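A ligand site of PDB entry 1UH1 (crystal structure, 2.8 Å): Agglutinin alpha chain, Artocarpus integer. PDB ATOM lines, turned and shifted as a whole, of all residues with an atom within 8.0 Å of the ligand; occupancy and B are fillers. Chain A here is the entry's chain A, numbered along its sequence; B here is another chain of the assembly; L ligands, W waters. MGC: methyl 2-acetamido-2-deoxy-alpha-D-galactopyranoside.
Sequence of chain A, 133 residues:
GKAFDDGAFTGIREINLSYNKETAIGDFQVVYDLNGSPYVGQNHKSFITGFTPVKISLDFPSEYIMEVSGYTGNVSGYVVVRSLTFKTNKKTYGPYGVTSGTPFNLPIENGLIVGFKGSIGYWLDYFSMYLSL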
ATOM      1  N   GLY A   1       6.410  11.578   2.485  1.00  0.00           N
ATOM      2  CA  GLY A   1       7.487  12.023   3.402  1.00  0.00           C
ATOM      3  C   GLY A   1       7.686  11.026   4.525  1.00  0.00           C
ATOM      4  O   GLY A   1       6.960  10.038   4.602  1.00  0.00           O
ATOM      5  N   LYS A   2       8.658  11.266   5.387  1.00  0.00           N
ATOM      6  CA  LYS A   2       8.889  10.345   6.486  1.00  0.00           C
ATOM      7  C   LYS A   2       8.049  10.739   7.687  1.00  0.00           C
ATOM      8  O   LYS A   2       8.160  11.862   8.198  1.00  0.00           O
ATOM      9  CB  LYS A   2      10.350  10.337   6.876  1.00  0.00           C
ATOM     10  CG  LYS A   2      10.537   9.442   8.034  1.00  0.00           C
ATOM     11  CD  LYS A   2      11.936   9.214   8.414  1.00  0.00           C
ATOM     12  CE  LYS A   2      11.922   8.056   9.377  1.00  0.00           C
ATOM     13  NZ  LYS A   2      13.252   7.857   9.980  1.00  0.00           N
ATOM     14  N   ALA A   3       7.218   9.813   8.141  1.00  0.00           N
ATOM     15  CA  ALA A   3       6.345  10.051   9.280  1.00  0.00           C
ATOM     16  C   ALA A   3       7.066  10.071  10.620  1.00  0.00           C
ATOM     17  O   ALA A   3       8.114   9.450  10.776  1.00  0.00           O
ATOM     18  CB  ALA A   3       5.260   8.996   9.314  1.00  0.00           C
ATOM     19  N   ALA A  24       7.028  26.223   1.780  1.00  0.00           N
ATOM     20  CA  ALA A  24       6.268  25.850   2.965  1.00  0.00           C
ATOM     21  C   ALA A  24       7.155  25.605   4.169  1.00  0.00           C
ATOM     22  O   ALA A  24       8.297  26.051   4.208  1.00  0.00           O
ATOM     23  CB  ALA A  24       5.446  24.596   2.662  1.00  0.00           C
ATOM     24  N   ILE A  25       6.613  24.897   5.154  1.00  0.00           N
ATOM     25  CA  ILE A  25       7.359  24.605   6.371  1.00  0.00           C
ATOM     26  C   ILE A  25       8.355  23.475   6.113  1.00  0.00           C
ATOM     27  O   ILE A  25       8.037  22.486   5.449  1.00  0.00           O
ATOM     28  CB  ILE A  25       6.415  24.194   7.537  1.00  0.00           C
ATOM     29  CG1 ILE A  25       5.411  25.317   7.831  1.00  0.00           C
ATOM     30  CG2 ILE A  25       7.241  23.878   8.777  1.00  0.00           C
ATOM     31  CD1 ILE A  25       6.043  26.580   8.358  1.00  0.00           C
ATOM     32  N   GLY A  26       9.556  23.624   6.662  1.00  0.00           N
ATOM     33  CA  GLY A  26      10.594  22.614   6.459  1.00  0.00           C
ATOM     34  C   GLY A  26      10.808  21.664   7.615  1.00  0.00           C
ATOM     35  O   GLY A  26      10.132  20.646   7.699  1.00  0.00           O
ATOM     36  N   SER A  46      13.674  18.033   6.826  1.00  0.00           N
ATOM     37  CA  SER A  46      13.239  17.992   5.442  1.00  0.00           C
ATOM     38  C   SER A  46      14.266  17.235   4.623  1.00  0.00           C
ATOM     39  O   SER A  46      15.439  17.164   4.983  1.00  0.00           O
ATOM     40  CB  SER A  46      13.100  19.396   4.883  1.00  0.00           C
ATOM     41  OG  SER A  46      13.056  19.380   3.468  1.00  0.00           O
ATOM     42  N   PHE A  47      13.818  16.655   3.509  1.00  0.00           N
ATOM     43  CA  PHE A  47      14.720  15.931   2.635  1.00  0.00           C
ATOM     44  C   PHE A  47      15.675  16.905   1.962  1.00  0.00           C
ATOM     45  O   PHE A  47      16.741  16.513   1.499  1.00  0.00           O
ATOM     46  CB  PHE A  47      13.956  15.169   1.565  1.00  0.00           C
ATOM     47  CG  PHE A  47      13.111  14.036   2.096  1.00  0.00           C
ATOM     48  CD1 PHE A  47      13.273  13.582   3.400  1.00  0.00           C
ATOM     49  CD2 PHE A  47      12.166  13.428   1.287  1.00  0.00           C
ATOM     50  CE1 PHE A  47      12.519  12.524   3.879  1.00  0.00           C
ATOM     51  CE2 PHE A  47      11.401  12.367   1.757  1.00  0.00           C
ATOM     52  CZ  PHE A  47      11.572  11.922   3.057  1.00  0.00           C
ATOM     53  N   ILE A  48      15.291  18.178   1.909  1.00  0.00           N
ATOM     54  CA  ILE A  48      16.122  19.206   1.282  1.00  0.00           C
ATOM     55  C   ILE A  48      16.526  20.269   2.308  1.00  0.00           C
ATOM     56  O   ILE A  48      16.162  20.180   3.484  1.00  0.00           O
ATOM     57  CB  ILE A  48      15.381  19.889   0.119  1.00  0.00           C
ATOM     58  CG1 ILE A  48      14.137  20.615   0.648  1.00  0.00           C
ATOM     59  CG2 ILE A  48      14.957  18.836  -0.910  1.00  0.00           C
ATOM     60  CD1 ILE A  48      13.279  21.236  -0.433  1.00  0.00           C
ATOM     61  N   VAL A  75       2.110  22.632  -3.333  1.00  0.00           N
ATOM     62  CA  VAL A  75       3.483  22.984  -3.694  1.00  0.00           C
ATOM     63  C   VAL A  75       4.079  21.846  -4.503  1.00  0.00           C
ATOM     64  O   VAL A  75       4.280  20.746  -3.990  1.00  0.00           O
ATOM     65  CB  VAL A  75       4.348  23.225  -2.440  1.00  0.00           C
ATOM     66  CG1 VAL A  75       5.784  23.504  -2.842  1.00  0.00           C
ATOM     67  CG2 VAL A  75       3.791  24.400  -1.671  1.00  0.00           C
ATOM     68  N   SER A  76       4.373  22.111  -5.778  1.00  0.00           N
ATOM     69  CA  SER A  76       4.918  21.094  -6.665  1.00  0.00           C
ATOM     70  C   SER A  76       3.989  19.892  -6.717  1.00  0.00           C
ATOM     71  O   SER A  76       4.438  18.759  -6.794  1.00  0.00           O
ATOM     72  CB  SER A  76       6.312  20.645  -6.215  1.00  0.00           C
ATOM     73  OG  SER A  76       7.294  21.605  -6.558  1.00  0.00           O
ATOM     74  N   GLY A  77       2.692  20.156  -6.643  1.00  0.00           N
ATOM     75  CA  GLY A  77       1.728  19.079  -6.710  1.00  0.00           C
ATOM     76  C   GLY A  77       1.459  18.314  -5.437  1.00  0.00           C
ATOM     77  O   GLY A  77       0.650  17.385  -5.430  1.00  0.00           O
ATOM     78  N   TYR A  78       2.135  18.663  -4.349  1.00  0.00           N
ATOM     79  CA  TYR A  78       1.932  17.997  -3.070  1.00  0.00           C
ATOM     80  C   TYR A  78       1.197  18.932  -2.128  1.00  0.00           C
ATOM     81  O   TYR A  78       1.492  20.114  -2.065  1.00  0.00           O
ATOM     82  CB  TYR A  78       3.277  17.632  -2.421  1.00  0.00           C
ATOM     83  CG  TYR A  78       4.124  16.678  -3.225  1.00  0.00           C
ATOM     84  CD1 TYR A  78       3.887  15.303  -3.204  1.00  0.00           C
ATOM     85  CD2 TYR A  78       5.161  17.146  -4.044  1.00  0.00           C
ATOM     86  CE1 TYR A  78       4.651  14.412  -3.961  1.00  0.00           C
ATOM     87  CE2 TYR A  78       5.935  16.273  -4.810  1.00  0.00           C
ATOM     88  CZ  TYR A  78       5.669  14.903  -4.776  1.00  0.00           C
ATOM     89  OH  TYR A  78       6.425  14.021  -5.514  1.00  0.00           O
ATOM     90  N   VAL A  79       0.218  18.400  -1.408  1.00  0.00           N
ATOM     91  CA  VAL A  79      -0.511  19.216  -0.439  1.00  0.00           C
ATOM     92  C   VAL A  79       0.334  19.206   0.834  1.00  0.00           C
ATOM     93  O   VAL A  79       0.639  18.144   1.364  1.00  0.00           O
ATOM     94  CB  VAL A  79      -1.879  18.620  -0.119  1.00  0.00           C
ATOM     95  CG1 VAL A  79      -2.525  19.398   1.020  1.00  0.00           C
ATOM     96  CG2 VAL A  79      -2.758  18.679  -1.355  1.00  0.00           C
ATOM     97  N   VAL A  80       0.715  20.393   1.300  1.00  0.00           N
ATOM     98  CA  VAL A  80       1.547  20.489   2.488  1.00  0.00           C
ATOM     99  C   VAL A  80       1.122  21.628   3.409  1.00  0.00           C
ATOM    100  O   VAL A  80       0.227  22.394   3.089  1.00  0.00           O
ATOM    101  CB  VAL A  80       3.032  20.700   2.108  1.00  0.00           C
ATOM    102  CG1 VAL A  80       3.556  19.521   1.302  1.00  0.00           C
ATOM    103  CG2 VAL A  80       3.167  21.971   1.314  1.00  0.00           C
ATOM    104  N   VAL A  81       1.761  21.726   4.573  1.00  0.00           N
ATOM    105  CA  VAL A  81       1.464  22.785   5.514  1.00  0.00           C
ATOM    106  C   VAL A  81       2.401  23.921   5.124  1.00  0.00           C
ATOM    107  O   VAL A  81       3.600  23.875   5.416  1.00  0.00           O
ATOM    108  CB  VAL A  81       1.741  22.350   6.972  1.00  0.00           C
ATOM    109  CG1 VAL A  81       1.429  23.490   7.924  1.00  0.00           C
ATOM    110  CG2 VAL A  81       0.886  21.137   7.309  1.00  0.00           C
ATOM    111  N   SER A 119       4.302  14.213   9.291  1.00  0.00           N
ATOM    112  CA  SER A 119       5.138  13.675   8.238  1.00  0.00           C
ATOM    113  C   SER A 119       5.907  14.786   7.550  1.00  0.00           C
ATOM    114  O   SER A 119       5.415  15.893   7.381  1.00  0.00           O
ATOM    115  CB  SER A 119       4.269  12.922   7.241  1.00  0.00           C
ATOM    116  OG  SER A 119       5.055  12.429   6.164  1.00  0.00           O
ATOM    117  N   ILE A 120       7.131  14.467   7.136  1.00  0.00           N
ATOM    118  CA  ILE A 120       7.975  15.448   6.451  1.00  0.00           C
ATOM    119  C   ILE A 120       8.779  14.841   5.310  1.00  0.00           C
ATOM    120  O   ILE A 120       9.543  13.902   5.499  1.00  0.00           O
ATOM    121  CB  ILE A 120       8.959  16.119   7.437  1.00  0.00           C
ATOM    122  CG1 ILE A 120       8.197  16.823   8.554  1.00  0.00           C
ATOM    123  CG2 ILE A 120       9.839  17.123   6.705  1.00  0.00           C
ATOM    124  CD1 ILE A 120       9.112  17.422   9.599  1.00  0.00           C
ATOM    125  N   GLY A 121       8.592  15.397   4.119  1.00  0.00           N
ATOM    126  CA  GLY A 121       9.332  14.962   2.947  1.00  0.00           C
ATOM    127  C   GLY A 121      10.161  16.189   2.640  1.00  0.00           C
ATOM    128  O   GLY A 121      11.077  16.514   3.396  1.00  0.00           O
ATOM    129  N   TYR A 122       9.848  16.875   1.549  1.00  0.00           N
ATOM    130  CA  TYR A 122      10.544  18.106   1.222  1.00  0.00           C
ATOM    131  C   TYR A 122       9.977  19.137   2.193  1.00  0.00           C
ATOM    132  O   TYR A 122      10.675  20.052   2.640  1.00  0.00           O
ATOM    133  CB  TYR A 122      10.221  18.545  -0.200  1.00  0.00           C
ATOM    134  CG  TYR A 122      11.060  17.895  -1.261  1.00  0.00           C
ATOM    135  CD1 TYR A 122      11.456  16.569  -1.154  1.00  0.00           C
ATOM    136  CD2 TYR A 122      11.439  18.618  -2.398  1.00  0.00           C
ATOM    137  CE1 TYR A 122      12.213  15.978  -2.154  1.00  0.00           C
ATOM    138  CE2 TYR A 122      12.187  18.027  -3.398  1.00  0.00           C
ATOM    139  CZ  TYR A 122      12.574  16.709  -3.271  1.00  0.00           C
ATOM    140  OH  TYR A 122      13.323  16.141  -4.269  1.00  0.00           O
ATOM    141  N   TRP A 123       8.699  18.968   2.500  1.00  0.00           N
ATOM    142  CA  TRP A 123       7.998  19.863   3.400  1.00  0.00           C
ATOM    143  C   TRP A 123       7.142  19.087   4.394  1.00  0.00           C
ATOM    144  O   TRP A 123       6.990  17.859   4.279  1.00  0.00           O
ATOM    145  CB  TRP A 123       7.129  20.810   2.577  1.00  0.00           C
ATOM    146  CG  TRP A 123       7.918  21.535   1.537  1.00  0.00           C
ATOM    147  CD1 TRP A 123       8.841  22.524   1.754  1.00  0.00           C
ATOM    148  CD2 TRP A 123       7.923  21.291   0.124  1.00  0.00           C
ATOM    149  NE1 TRP A 123       9.409  22.908   0.564  1.00  0.00           N
ATOM    150  CE2 TRP A 123       8.861  22.156  -0.447  1.00  0.00           C
ATOM    151  CE3 TRP A 123       7.204  20.412  -0.705  1.00  0.00           C
ATOM    152  CZ2 TRP A 123       9.115  22.188  -1.816  1.00  0.00           C
ATOM    153  CZ3 TRP A 123       7.458  20.434  -2.070  1.00  0.00           C
ATOM    154  CH2 TRP A 123       8.410  21.323  -2.609  1.00  0.00           C
ATOM    155  N   LEU A 124       6.600  19.797   5.376  1.00  0.00           N
ATOM    156  CA  LEU A 124       5.742  19.205   6.368  1.00  0.00           C
ATOM    157  C   LEU A 124       4.453  18.818   5.635  1.00  0.00           C
ATOM    158  O   LEU A 124       3.659  19.672   5.267  1.00  0.00           O
ATOM    159  CB  LEU A 124       5.457  20.221   7.467  1.00  0.00           C
ATOM    160  CG  LEU A 124       4.481  19.856   8.585  1.00  0.00           C
ATOM    161  CD1 LEU A 124       4.947  18.613   9.336  1.00  0.00           C
ATOM    162  CD2 LEU A 124       4.372  21.043   9.529  1.00  0.00           C
ATOM    163  N   ASP A 125       4.259  17.518   5.425  1.00  0.00           N
ATOM    164  CA  ASP A 125       3.077  17.020   4.715  1.00  0.00           C
ATOM    165  C   ASP A 125       1.798  17.229   5.485  1.00  0.00           C
ATOM    166  O   ASP A 125       0.796  17.672   4.930  1.00  0.00           O
ATOM    167  CB  ASP A 125       3.248  15.545   4.407  1.00  0.00           C
ATOM    168  CG  ASP A 125       4.502  15.257   3.629  1.00  0.00           C
ATOM    169  OD1 ASP A 125       4.646  15.829   2.537  1.00  0.00           O
ATOM    170  OD2 ASP A 125       5.351  14.487   4.120  1.00  0.00           O
ATOM    171  N   TYR A 126       1.834  16.900   6.772  1.00  0.00           N
ATOM    172  CA  TYR A 126       0.670  17.056   7.628  1.00  0.00           C
ATOM    173  C   TYR A 126       1.108  16.870   9.063  1.00  0.00           C
ATOM    174  O   TYR A 126       2.234  16.431   9.319  1.00  0.00           O
ATOM    175  CB  TYR A 126      -0.387  16.015   7.283  1.00  0.00           C
ATOM    176  CG  TYR A 126       0.100  14.604   7.448  1.00  0.00           C
ATOM    177  CD1 TYR A 126       0.263  14.036   8.713  1.00  0.00           C
ATOM    178  CD2 TYR A 126       0.426  13.829   6.332  1.00  0.00           C
ATOM    179  CE1 TYR A 126       0.735  12.742   8.874  1.00  0.00           C
ATOM    180  CE2 TYR A 126       0.906  12.536   6.470  1.00  0.00           C
ATOM    181  CZ  TYR A 126       1.060  11.991   7.737  1.00  0.00           C
ATOM    182  OH  TYR A 126       1.521  10.699   7.877  1.00  0.00           O
ATOM    183  N   ALA B  17      -1.577  17.311   3.965  1.00  0.00           N
ATOM    184  CA  ALA B  17      -1.751  16.175   3.085  1.00  0.00           C
ATOM    185  C   ALA B  17      -2.652  15.133   3.726  1.00  0.00           C
ATOM    186  O   ALA B  17      -2.412  14.726   4.860  1.00  0.00           O
ATOM    187  CB  ALA B  17      -0.422  15.570   2.769  1.00  0.00           C
HETATM  188  O6  MGC L   1       6.613  17.301   1.428  1.00  0.00           O
HETATM  189  C6  MGC L   1       6.273  16.646   0.214  1.00  0.00           C
HETATM  190  C5  MGC L   1       6.596  15.348  -0.522  1.00  0.00           C
HETATM  191  O5  MGC L   1       8.026  15.134  -0.598  1.00  0.00           O
HETATM  192  C1  MGC L   1       8.490  13.969  -1.295  1.00  0.00           C
HETATM  193  O1  MGC L   1       8.422  14.226  -2.680  1.00  0.00           O
HETATM  194  CM  MGC L   1       9.101  14.947  -3.707  1.00  0.00           C
HETATM  195  C2  MGC L   1       7.844  12.722  -0.618  1.00  0.00           C
HETATM  196  N2  MGC L   1       8.126  11.501  -1.403  1.00  0.00           N
HETATM  197  C7  MGC L   1       8.702  10.487  -0.673  1.00  0.00           C
HETATM  198  O7  MGC L   1       8.972  10.554   0.533  1.00  0.00           O
HETATM  199  C8  MGC L   1       9.015   9.204  -1.424  1.00  0.00           C
HETATM  200  C3  MGC L   1       6.307  12.862  -0.565  1.00  0.00           C
HETATM  201  O3  MGC L   1       5.731  11.727   0.047  1.00  0.00           O
HETATM  202  C4  MGC L   1       5.935  14.139   0.195  1.00  0.00           C
HETATM  203  O4  MGC L   1       6.331  14.050   1.550  1.00  0.00           O
HETATM  204  O   HOH W   1       3.175  11.831  -0.744  1.00  0.00           O
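The side-chain hydroxyl (OH) of Tyr 78 lies close to an oxygen (O1) of the ligand (3.5 Å).
N of Gly 1 lies within hydrogen-bond range of O3 of the ligand (2.5 Å).
O of Trp 123 is in hydrogen-bond range of O6 of the ligand, at 2.9 Å.
The side-chain carboxylate of Asp 125 lies within hydrogen-bond range of an oxygen (O4) of the ligand, at 2.6 Å.
N of Tyr 122 lies within hydrogen-bond range of O6 of the ligand (3.3 Å).
N of Trp 123 lies within hydrogen-bond range of O6 of the ligand, at 2.9 Å.
The backbone NH of Phe 47 is in hydrogen-bond range of the backbone carbonyl oxygen of Gly 121, at 2.7 Å.
O of Gly 121 lies close to OG of Ser 46.
The side-chain carboxylate (OD2) of Asp 125 lies within hydrogen-bond range of the backbone NH (N) of Gly 121 (3.4 Å).
The side-chain hydroxyl (OG) of Ser 46 lies within hydrogen-bond range of the backbone carbonyl oxygen (O) of Tyr 122 (2.6 Å).
The backbone carbonyl oxygen (O) of Ser 119 sits at hydrogen-bond distance from the backbone NH (N) of Asp 125 (2.8 Å).
The side-chain hydroxyl (OG) of Ser 119 lies close to the backbone carbonyl oxygen (O) of Gly 1 (3.4 Å).
The backbone carbonyl oxygen of Asp 125 is in hydrogen-bond range of the backbone NH of Ala 17 of chain B.
Residues that only touch the ligand: Phe 47 (3.3 Å), Gly 121 (3.4 Å) and Val 80 (3.8 Å).
Hydrophobic or aromatic side chains within 4 Å of the ligand: Phe 47, Tyr 78, Val 80, Tyr 122 and Trp 123.
Along chain A the residues within 4 Å of the ligand span positions 1 to 125.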
